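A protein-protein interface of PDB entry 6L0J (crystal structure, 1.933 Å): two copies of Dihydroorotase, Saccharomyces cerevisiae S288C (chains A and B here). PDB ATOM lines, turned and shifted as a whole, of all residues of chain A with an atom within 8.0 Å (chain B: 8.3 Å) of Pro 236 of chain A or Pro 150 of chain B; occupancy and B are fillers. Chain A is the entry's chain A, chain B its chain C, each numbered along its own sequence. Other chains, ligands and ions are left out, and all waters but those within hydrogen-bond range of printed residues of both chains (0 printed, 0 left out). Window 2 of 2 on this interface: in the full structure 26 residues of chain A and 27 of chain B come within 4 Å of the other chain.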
ATOM      1  N   GLU A 184      10.922  24.593  24.474  1.00  0.00           N
ATOM      2  CA  GLU A 184      11.065  23.269  25.070  1.00  0.00           C
ATOM      3  C   GLU A 184       9.902  22.959  26.007  1.00  0.00           C
ATOM      4  O   GLU A 184       9.376  21.841  26.002  1.00  0.00           O
ATOM      5  CB  GLU A 184      12.402  23.184  25.822  1.00  0.00           C
ATOM      6  CG  GLU A 184      12.582  21.900  26.625  1.00  0.00           C
ATOM      7  CD  GLU A 184      13.980  21.751  27.234  1.00  0.00           C
ATOM      8  OE1 GLU A 184      14.568  20.680  27.058  1.00  0.00           O
ATOM      9  OE2 GLU A 184      14.493  22.690  27.885  1.00  0.00           O
ATOM     10  N   LEU A 216      16.105  29.110  13.614  1.00  0.00           N
ATOM     11  CA  LEU A 216      16.341  30.420  14.203  1.00  0.00           C
ATOM     12  C   LEU A 216      16.469  30.352  15.710  1.00  0.00           C
ATOM     13  O   LEU A 216      15.825  29.544  16.367  1.00  0.00           O
ATOM     14  CB  LEU A 216      15.210  31.393  13.857  1.00  0.00           C
ATOM     15  CG  LEU A 216      14.991  31.649  12.371  1.00  0.00           C
ATOM     16  CD1 LEU A 216      13.706  32.441  12.167  1.00  0.00           C
ATOM     17  CD2 LEU A 216      16.175  32.390  11.789  1.00  0.00           C
ATOM     18  N   THR A 217      17.285  31.255  16.257  1.00  0.00           N
ATOM     19  CA  THR A 217      17.254  31.614  17.664  1.00  0.00           C
ATOM     20  C   THR A 217      17.141  33.133  17.769  1.00  0.00           C
ATOM     21  O   THR A 217      17.154  33.850  16.757  1.00  0.00           O
ATOM     22  CB  THR A 217      18.503  31.121  18.401  1.00  0.00           C
ATOM     23  OG1 THR A 217      19.621  31.938  18.019  1.00  0.00           O
ATOM     24  CG2 THR A 217      18.793  29.659  18.056  1.00  0.00           C
ATOM     25  N   ILE A 218      17.066  33.623  19.009  1.00  0.00           N
ATOM     26  CA  ILE A 218      16.883  35.056  19.247  1.00  0.00           C
ATOM     27  C   ILE A 218      17.996  35.864  18.598  1.00  0.00           C
ATOM     28  O   ILE A 218      17.773  36.997  18.153  1.00  0.00           O
ATOM     29  CB  ILE A 218      16.779  35.356  20.757  1.00  0.00           C
ATOM     30  CG1 ILE A 218      16.655  36.860  21.002  1.00  0.00           C
ATOM     31  CG2 ILE A 218      17.994  34.806  21.507  1.00  0.00           C
ATOM     32  CD1 ILE A 218      16.008  37.228  22.346  1.00  0.00           C
ATOM     33  N   ASP A 219      19.201  35.295  18.504  1.00  0.00           N
ATOM     34  CA  ASP A 219      20.307  36.013  17.876  1.00  0.00           C
ATOM     35  C   ASP A 219      20.063  36.292  16.400  1.00  0.00           C
ATOM     36  O   ASP A 219      20.646  37.231  15.853  1.00  0.00           O
ATOM     37  CB  ASP A 219      21.611  35.228  18.037  1.00  0.00           C
ATOM     38  CG  ASP A 219      22.293  35.495  19.368  1.00  0.00           C
ATOM     39  OD1 ASP A 219      23.530  35.365  19.427  1.00  0.00           O
ATOM     40  OD2 ASP A 219      21.595  35.823  20.353  1.00  0.00           O
ATOM     41  N   ALA A 233      11.377  33.257  17.894  1.00  0.00           N
ATOM     42  CA  ALA A 233      12.394  32.237  18.098  1.00  0.00           C
ATOM     43  C   ALA A 233      13.148  32.525  19.392  1.00  0.00           C
ATOM     44  O   ALA A 233      13.488  33.676  19.695  1.00  0.00           O
ATOM     45  CB  ALA A 233      13.370  32.197  16.911  1.00  0.00           C
ATOM     46  N   LYS A 234      13.421  31.474  20.157  1.00  0.00           N
ATOM     47  CA  LYS A 234      13.885  31.682  21.525  1.00  0.00           C
ATOM     48  C   LYS A 234      15.338  31.234  21.673  1.00  0.00           C
ATOM     49  O   LYS A 234      16.170  31.586  20.833  1.00  0.00           O
ATOM     50  CB  LYS A 234      12.919  30.986  22.489  1.00  0.00           C
ATOM     51  CG  LYS A 234      11.534  31.681  22.418  1.00  0.00           C
ATOM     52  CD  LYS A 234      10.427  30.899  23.090  1.00  0.00           C
ATOM     53  CE  LYS A 234       9.222  31.795  23.268  1.00  0.00           C
ATOM     54  NZ  LYS A 234       8.463  32.024  21.984  1.00  0.00           N
ATOM     55  N   LEU A 235      15.657  30.447  22.712  1.00  0.00           N
ATOM     56  CA  LEU A 235      17.049  30.188  23.062  1.00  0.00           C
ATOM     57  C   LEU A 235      17.578  28.959  22.340  1.00  0.00           C
ATOM     58  O   LEU A 235      16.808  28.147  21.823  1.00  0.00           O
ATOM     59  CB  LEU A 235      17.178  30.010  24.577  1.00  0.00           C
ATOM     60  CG  LEU A 235      16.684  31.188  25.423  1.00  0.00           C
ATOM     61  CD1 LEU A 235      17.051  31.027  26.892  1.00  0.00           C
ATOM     62  CD2 LEU A 235      17.247  32.484  24.878  1.00  0.00           C
ATOM     63  N   PRO A 236      18.912  28.809  22.246  1.00  0.00           N
ATOM     64  CA  PRO A 236      19.468  27.559  21.687  1.00  0.00           C
ATOM     65  C   PRO A 236      18.841  26.305  22.258  1.00  0.00           C
ATOM     66  O   PRO A 236      18.607  25.342  21.518  1.00  0.00           O
ATOM     67  CB  PRO A 236      20.955  27.648  22.049  1.00  0.00           C
ATOM     68  CG  PRO A 236      21.227  29.136  22.040  1.00  0.00           C
ATOM     69  CD  PRO A 236      19.967  29.794  22.557  1.00  0.00           C
ATOM     70  N   ASN A 237      18.554  26.290  23.557  1.00  0.00           N
ATOM     71  CA  ASN A 237      17.979  25.082  24.140  1.00  0.00           C
ATOM     72  C   ASN A 237      16.581  24.820  23.608  1.00  0.00           C
ATOM     73  O   ASN A 237      16.207  23.659  23.427  1.00  0.00           O
ATOM     74  CB  ASN A 237      17.953  25.173  25.673  1.00  0.00           C
ATOM     75  CG  ASN A 237      17.322  23.953  26.313  1.00  0.00           C
ATOM     76  OD1 ASN A 237      17.955  22.903  26.422  1.00  0.00           O
ATOM     77  ND2 ASN A 237      16.057  24.073  26.712  1.00  0.00           N
ATOM     78  N   ASP A 238      15.797  25.875  23.342  1.00  0.00           N
ATOM     79  CA  ASP A 238      14.460  25.681  22.773  1.00  0.00           C
ATOM     80  C   ASP A 238      14.547  25.127  21.356  1.00  0.00           C
ATOM     81  O   ASP A 238      13.902  24.124  21.027  1.00  0.00           O
ATOM     82  CB  ASP A 238      13.679  26.996  22.783  1.00  0.00           C
ATOM     83  CG  ASP A 238      13.448  27.533  24.194  1.00  0.00           C
ATOM     84  OD1 ASP A 238      12.684  26.895  24.952  1.00  0.00           O
ATOM     85  OD2 ASP A 238      14.031  28.582  24.546  1.00  0.00           O
ATOM     86  N   LYS A 239      15.354  25.762  20.506  1.00  0.00           N
ATOM     87  CA  LYS A 239      15.541  25.274  19.144  1.00  0.00           C
ATOM     88  C   LYS A 239      15.942  23.799  19.119  1.00  0.00           C
ATOM     89  O   LYS A 239      15.407  23.020  18.325  1.00  0.00           O
ATOM     90  CB  LYS A 239      16.590  26.129  18.417  1.00  0.00           C
ATOM     91  CG  LYS A 239      17.065  25.492  17.107  1.00  0.00           C
ATOM     92  CD  LYS A 239      17.856  26.454  16.219  1.00  0.00           C
ATOM     93  CE  LYS A 239      19.345  26.189  16.310  1.00  0.00           C
ATOM     94  NZ  LYS A 239      20.090  26.778  15.166  1.00  0.00           N
ATOM     95  N   LYS A 240      16.899  23.397  19.976  1.00  0.00           N
ATOM     96  CA  LYS A 240      17.299  21.990  20.038  1.00  0.00           C
ATOM     97  C   LYS A 240      16.100  21.088  20.303  1.00  0.00           C
ATOM     98  O   LYS A 240      15.965  20.014  19.699  1.00  0.00           O
ATOM     99  CB  LYS A 240      18.369  21.777  21.121  1.00  0.00           C
ATOM    100  CG  LYS A 240      18.743  20.282  21.390  1.00  0.00           C
ATOM    101  CD  LYS A 240      19.854  20.119  22.485  1.00  0.00           C
ATOM    102  CE  LYS A 240      19.914  18.686  23.041  1.00  0.00           C
ATOM    103  NZ  LYS A 240      18.662  18.306  23.796  1.00  0.00           N
ATOM    104  N   ALA A 241      15.228  21.503  21.216  1.00  0.00           N
ATOM    105  CA  ALA A 241      14.072  20.687  21.565  1.00  0.00           C
ATOM    106  C   ALA A 241      13.042  20.641  20.440  1.00  0.00           C
ATOM    107  O   ALA A 241      12.374  19.616  20.266  1.00  0.00           O
ATOM    108  CB  ALA A 241      13.436  21.204  22.852  1.00  0.00           C
ATOM    109  N   LEU A 242      12.902  21.723  19.664  1.00  0.00           N
ATOM    110  CA  LEU A 242      12.008  21.688  18.505  1.00  0.00           C
ATOM    111  C   LEU A 242      12.537  20.755  17.425  1.00  0.00           C
ATOM    112  O   LEU A 242      11.779  19.972  16.834  1.00  0.00           O
ATOM    113  CB  LEU A 242      11.833  23.090  17.925  1.00  0.00           C
ATOM    114  CG  LEU A 242      11.437  24.186  18.900  1.00  0.00           C
ATOM    115  CD1 LEU A 242      11.309  25.548  18.141  1.00  0.00           C
ATOM    116  CD2 LEU A 242      10.138  23.793  19.589  1.00  0.00           C
ATOM    117  N   VAL A 243      13.839  20.848  17.137  1.00  0.00           N
ATOM    118  CA  VAL A 243      14.446  19.971  16.136  1.00  0.00           C
ATOM    119  C   VAL A 243      14.272  18.519  16.548  1.00  0.00           C
ATOM    120  O   VAL A 243      13.895  17.657  15.745  1.00  0.00           O
ATOM    121  CB  VAL A 243      15.937  20.305  15.948  1.00  0.00           C
ATOM    122  CG1 VAL A 243      16.658  19.154  15.242  1.00  0.00           C
ATOM    123  CG2 VAL A 243      16.129  21.585  15.148  1.00  0.00           C
ATOM    124  N   PRO B 141      31.238  37.590  22.576  1.00  0.00           N
ATOM    125  CA  PRO B 141      30.644  37.358  21.257  1.00  0.00           C
ATOM    126  C   PRO B 141      29.822  36.080  21.266  1.00  0.00           C
ATOM    127  O   PRO B 141      30.092  35.151  22.030  1.00  0.00           O
ATOM    128  CB  PRO B 141      31.862  37.234  20.333  1.00  0.00           C
ATOM    129  CG  PRO B 141      32.987  37.869  21.090  1.00  0.00           C
ATOM    130  CD  PRO B 141      32.710  37.600  22.527  1.00  0.00           C
ATOM    131  N   SER B 142      28.795  36.049  20.421  1.00  0.00           N
ATOM    132  CA  SER B 142      27.880  34.915  20.413  1.00  0.00           C
ATOM    133  C   SER B 142      28.555  33.697  19.784  1.00  0.00           C
ATOM    134  O   SER B 142      29.465  33.820  18.961  1.00  0.00           O
ATOM    135  CB  SER B 142      26.596  35.276  19.665  1.00  0.00           C
ATOM    136  OG  SER B 142      25.855  36.274  20.363  1.00  0.00           O
ATOM    137  N   VAL B 143      28.115  32.505  20.187  1.00  0.00           N
ATOM    138  CA  VAL B 143      28.834  31.280  19.844  1.00  0.00           C
ATOM    139  C   VAL B 143      27.840  30.191  19.447  1.00  0.00           C
ATOM    140  O   VAL B 143      26.916  29.872  20.201  1.00  0.00           O
ATOM    141  CB  VAL B 143      29.740  30.825  21.009  1.00  0.00           C
ATOM    142  CG1 VAL B 143      30.217  29.405  20.804  1.00  0.00           C
ATOM    143  CG2 VAL B 143      30.931  31.786  21.169  1.00  0.00           C
ATOM    144  N   HIS B 144      28.047  29.612  18.263  1.00  0.00           N
ATOM    145  CA  HIS B 144      27.163  28.617  17.664  1.00  0.00           C
ATOM    146  C   HIS B 144      27.609  27.198  18.023  1.00  0.00           C
ATOM    147  O   HIS B 144      27.138  26.625  19.013  1.00  0.00           O
ATOM    148  CB  HIS B 144      27.149  28.830  16.146  1.00  0.00           C
ATOM    149  CG  HIS B 144      26.227  27.919  15.398  1.00  0.00           C
ATOM    150  ND1 HIS B 144      24.866  28.132  15.327  1.00  0.00           N
ATOM    151  CD2 HIS B 144      26.473  26.811  14.661  1.00  0.00           C
ATOM    152  CE1 HIS B 144      24.312  27.185  14.590  1.00  0.00           C
ATOM    153  NE2 HIS B 144      25.265  26.370  14.174  1.00  0.00           N
ATOM    154  N   ASP B 145      28.492  26.622  17.203  1.00  0.00           N
ATOM    155  CA  ASP B 145      29.271  25.429  17.528  1.00  0.00           C
ATOM    156  C   ASP B 145      28.449  24.164  17.765  1.00  0.00           C
ATOM    157  O   ASP B 145      28.014  23.507  16.816  1.00  0.00           O
ATOM    158  CB  ASP B 145      30.138  25.695  18.757  1.00  0.00           C
ATOM    159  CG  ASP B 145      31.252  26.688  18.489  1.00  0.00           C
ATOM    160  OD1 ASP B 145      31.460  27.052  17.304  1.00  0.00           O
ATOM    161  OD2 ASP B 145      31.929  27.092  19.463  1.00  0.00           O
ATOM    162  N   GLY B 146      28.274  23.789  19.029  1.00  0.00           N
ATOM    163  CA  GLY B 146      27.609  22.547  19.381  1.00  0.00           C
ATOM    164  C   GLY B 146      28.345  21.753  20.448  1.00  0.00           C
ATOM    165  O   GLY B 146      27.912  20.652  20.829  1.00  0.00           O
ATOM    166  N   ASP B 147      29.463  22.308  20.928  1.00  0.00           N
ATOM    167  CA  ASP B 147      30.259  21.713  22.000  1.00  0.00           C
ATOM    168  C   ASP B 147      30.205  22.559  23.267  1.00  0.00           C
ATOM    169  O   ASP B 147      29.770  22.083  24.323  1.00  0.00           O
ATOM    170  CB  ASP B 147      31.717  21.530  21.532  1.00  0.00           C
ATOM    171  CG  ASP B 147      32.639  20.995  22.627  1.00  0.00           C
ATOM    172  OD1 ASP B 147      32.893  19.770  22.662  1.00  0.00           O
ATOM    173  OD2 ASP B 147      33.130  21.799  23.448  1.00  0.00           O
ATOM    174  N   LYS B 148      30.617  23.822  23.178  1.00  0.00           N
ATOM    175  CA  LYS B 148      30.691  24.733  24.311  1.00  0.00           C
ATOM    176  C   LYS B 148      29.380  25.484  24.498  1.00  0.00           C
ATOM    177  O   LYS B 148      28.673  25.793  23.538  1.00  0.00           O
ATOM    178  CB  LYS B 148      31.847  25.721  24.124  1.00  0.00           C
ATOM    179  CG  LYS B 148      32.554  26.106  25.409  1.00  0.00           C
ATOM    180  CD  LYS B 148      32.068  27.454  25.931  1.00  0.00           C
ATOM    181  CE  LYS B 148      32.827  27.862  27.189  1.00  0.00           C
ATOM    182  NZ  LYS B 148      31.938  28.622  28.115  1.00  0.00           N
ATOM    183  N   GLU B 149      29.067  25.779  25.765  1.00  0.00           N
ATOM    184  CA  GLU B 149      27.831  26.391  26.236  1.00  0.00           C
ATOM    185  C   GLU B 149      27.395  27.583  25.382  1.00  0.00           C
ATOM    186  O   GLU B 149      28.215  28.441  25.026  1.00  0.00           O
ATOM    187  CB  GLU B 149      27.987  26.824  27.696  1.00  0.00           C
ATOM    188  CG  GLU B 149      26.681  27.027  28.413  1.00  0.00           C
ATOM    189  CD  GLU B 149      26.865  27.821  29.686  1.00  0.00           C
ATOM    190  OE1 GLU B 149      27.342  28.984  29.609  1.00  0.00           O
ATOM    191  OE2 GLU B 149      26.531  27.281  30.765  1.00  0.00           O
ATOM    192  N   PRO B 150      26.116  27.659  25.028  1.00  0.00           N
ATOM    193  CA  PRO B 150      25.668  28.713  24.109  1.00  0.00           C
ATOM    194  C   PRO B 150      25.788  30.119  24.696  1.00  0.00           C
ATOM    195  O   PRO B 150      25.525  30.344  25.877  1.00  0.00           O
ATOM    196  CB  PRO B 150      24.212  28.334  23.837  1.00  0.00           C
ATOM    197  CG  PRO B 150      24.199  26.846  23.989  1.00  0.00           C
ATOM    198  CD  PRO B 150      25.145  26.554  25.123  1.00  0.00           C
ATOM    199  N   ILE B 151      26.207  31.058  23.844  1.00  0.00           N
ATOM    200  CA  ILE B 151      26.285  32.491  24.148  1.00  0.00           C
ATOM    201  C   ILE B 151      25.377  33.224  23.174  1.00  0.00           C
ATOM    202  O   ILE B 151      25.574  33.143  21.955  1.00  0.00           O
ATOM    203  CB  ILE B 151      27.716  33.042  24.028  1.00  0.00           C
ATOM    204  CG1 ILE B 151      28.669  32.308  24.968  1.00  0.00           C
ATOM    205  CG2 ILE B 151      27.734  34.553  24.291  1.00  0.00           C
ATOM    206  CD1 ILE B 151      28.178  32.256  26.370  1.00  0.00           C
ATOM    207  N   HIS B 152      24.410  33.967  23.703  1.00  0.00           N
ATOM    208  CA  HIS B 152      23.455  34.685  22.870  1.00  0.00           C
ATOM    209  C   HIS B 152      23.233  36.068  23.468  1.00  0.00           C
ATOM    210  O   HIS B 152      23.748  36.379  24.547  1.00  0.00           O
ATOM    211  CB  HIS B 152      22.152  33.902  22.768  1.00  0.00           C
ATOM    212  CG  HIS B 152      21.694  33.358  24.076  1.00  0.00           C
ATOM    213  ND1 HIS B 152      21.013  34.122  24.998  1.00  0.00           N
ATOM    214  CD2 HIS B 152      21.854  32.139  24.638  1.00  0.00           C
ATOM    215  CE1 HIS B 152      20.752  33.389  26.065  1.00  0.00           C
ATOM    216  NE2 HIS B 152      21.251  32.180  25.871  1.00  0.00           N
ATOM    217  N   VAL B 153      22.450  36.901  22.768  1.00  0.00           N
ATOM    218  CA  VAL B 153      22.249  38.287  23.207  1.00  0.00           C
ATOM    219  C   VAL B 153      21.661  38.374  24.613  1.00  0.00           C
ATOM    220  O   VAL B 153      21.824  39.400  25.281  1.00  0.00           O
ATOM    221  CB  VAL B 153      21.359  39.087  22.220  1.00  0.00           C
ATOM    222  CG1 VAL B 153      22.074  39.322  20.907  1.00  0.00           C
ATOM    223  CG2 VAL B 153      20.007  38.408  21.998  1.00  0.00           C
ATOM    224  N   LEU B 154      20.980  37.333  25.099  1.00  0.00           N
ATOM    225  CA  LEU B 154      20.404  37.468  26.434  1.00  0.00           C
ATOM    226  C   LEU B 154      21.364  37.066  27.555  1.00  0.00           C
ATOM    227  O   LEU B 154      21.195  37.527  28.686  1.00  0.00           O
ATOM    228  CB  LEU B 154      19.105  36.664  26.554  1.00  0.00           C
ATOM    229  CG  LEU B 154      18.031  37.172  25.601  1.00  0.00           C
ATOM    230  CD1 LEU B 154      16.920  36.156  25.596  1.00  0.00           C
ATOM    231  CD2 LEU B 154      17.542  38.565  26.023  1.00  0.00           C
ATOM    232  N   ASN B 155      22.360  36.222  27.290  1.00  0.00           N
ATOM    233  CA  ASN B 155      23.315  35.818  28.322  1.00  0.00           C
ATOM    234  C   ASN B 155      24.753  36.250  28.026  1.00  0.00           C
ATOM    235  O   ASN B 155      25.667  35.849  28.754  1.00  0.00           O
ATOM    236  CB  ASN B 155      23.267  34.294  28.536  1.00  0.00           C
ATOM    237  CG  ASN B 155      23.932  33.497  27.414  1.00  0.00           C
ATOM    238  OD1 ASN B 155      24.292  34.022  26.369  1.00  0.00           O
ATOM    239  ND2 ASN B 155      24.086  32.188  27.642  1.00  0.00           N
ATOM    240  N   ALA B 156      24.982  37.043  26.976  1.00  0.00           N
ATOM    241  CA  ALA B 156      26.343  37.432  26.628  1.00  0.00           C
ATOM    242  C   ALA B 156      26.952  38.338  27.692  1.00  0.00           C
ATOM    243  O   ALA B 156      28.157  38.266  27.953  1.00  0.00           O
ATOM    244  CB  ALA B 156      26.354  38.115  25.261  1.00  0.00           C
ATOM    245  N   ALA B 159      27.857  36.045  30.668  1.00  0.00           N
ATOM    246  CA  ALA B 159      29.042  35.258  30.343  1.00  0.00           C
ATOM    247  C   ALA B 159      30.320  36.089  30.378  1.00  0.00           C
ATOM    248  O   ALA B 159      31.410  35.525  30.516  1.00  0.00           O
ATOM    249  CB  ALA B 159      28.886  34.617  28.966  1.00  0.00           C
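Hydrophobic or aromatic side chains of chain B within 4 Å of the printed part of chain A: Pro 150, His 152, Val 153 and Leu 154. Of the 16 printed residues of chain A, 4 touch a printed residue of chain B. Printed residues of chain A that touch a printed residue of chain B: Ile 218, Asp 219, Leu 235 and Pro 236. Hydrophobic or aromatic side chains of chain A within 4 Å of the printed part of chain B: Ile 218, Leu 235 and Pro 236. Along chain A the printed residues that touch a printed residue of chain B span positions 218 to 236. Among the printed residues, no Asp or Glu carboxylate lies within 4 Å of a Lys or Arg side-chain nitrogen of the other chain.
Pro 236 of chain A touches just these residues of chain B: Pro 150 (3.6 Å) and His 152 (3.7 Å). Of chain A, only Pro 236 comes within 4 Å of Pro 150 of chain B. Printed residues of chain B within 4 Å of Ile 218 of chain A: Val 153 and Leu 154. Of the printed residues of chain A, Ile 151 of chain B touches Asp 219 (3.9 Å). Of the printed residues of chain B, Asp 219 of chain A touches Ser 142 (2.7 Å), Ile 151 (3.9 Å), His 152 (3.1 Å) and Val 153 (2.8 Å). Printed residues of chain A within 4 Å of Leu 154 of chain B: Ile 218 and Leu 235. The nearest residue of chain A that does not touch Pro 150 of chain B is Asn 237 of chain A (5.7 Å). The nearest printed residue of chain B that does not touch Ile 218 of chain A is His 152 of chain B (4.4 Å).
Among the printed residues, pairs that only touch across the chains: Ile 218 of chain A with Val 153 of chain B (3.8 Å), Ile 218 of chain A with Leu 154 of chain B (3.5 Å), Asp 219 of chain A with Ile 151 of chain B (3.9 Å), Asp 219 of chain A with His 152 of chain B (3.1 Å), Leu 235 of chain A with His 152 of chain B (3.8 Å), Leu 235 of chain A with Leu 154 of chain B (3.8 Å), Pro 236 of chain A with Pro 150 of chain B (3.6 Å) and Pro 236 of chain A with His 152 of chain B (3.7 Å).
The side-chain hydroxyl (OG1) of Thr 217 of chain A lies close to the backbone NH (N) of Asp 219 of chain A (3.4 Å). The backbone carbonyl oxygen of Lys 234 of chain A sits at hydrogen-bond distance from the backbone NH of Ile 218 of chain A (2.9 Å). OD2 of Asp 238 of chain A sits at hydrogen-bond distance from N of Leu 235 of chain A (3.1 Å). O of Ile 151 of chain B sits at hydrogen-bond distance from N of Val 143 of chain B (3.2 Å). The side-chain amide nitrogen (ND2) of Asn 155 of chain B is in hydrogen-bond range of the backbone carbonyl oxygen (O) of Pro 150 of chain B, 2.9 Å away. ND1 of His 152 of chain B sits close to N of Leu 154 of chain B (3.2 Å).
The side-chain hydroxyl (OG) of Ser 142 of chain B is in hydrogen-bond range of the side-chain carboxylate (OD1) of Asp 219 of chain A (2.7 Å). The side-chain carboxylate (OD2) of Asp 219 of chain A is in hydrogen-bond range of the backbone NH (N) of Val 153 of chain B (2.8 Å).
No position is printed for both chains. Of the 10 pairs that touch across the chains among the printed residues, none has its exchanged pair printed and touching as well.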
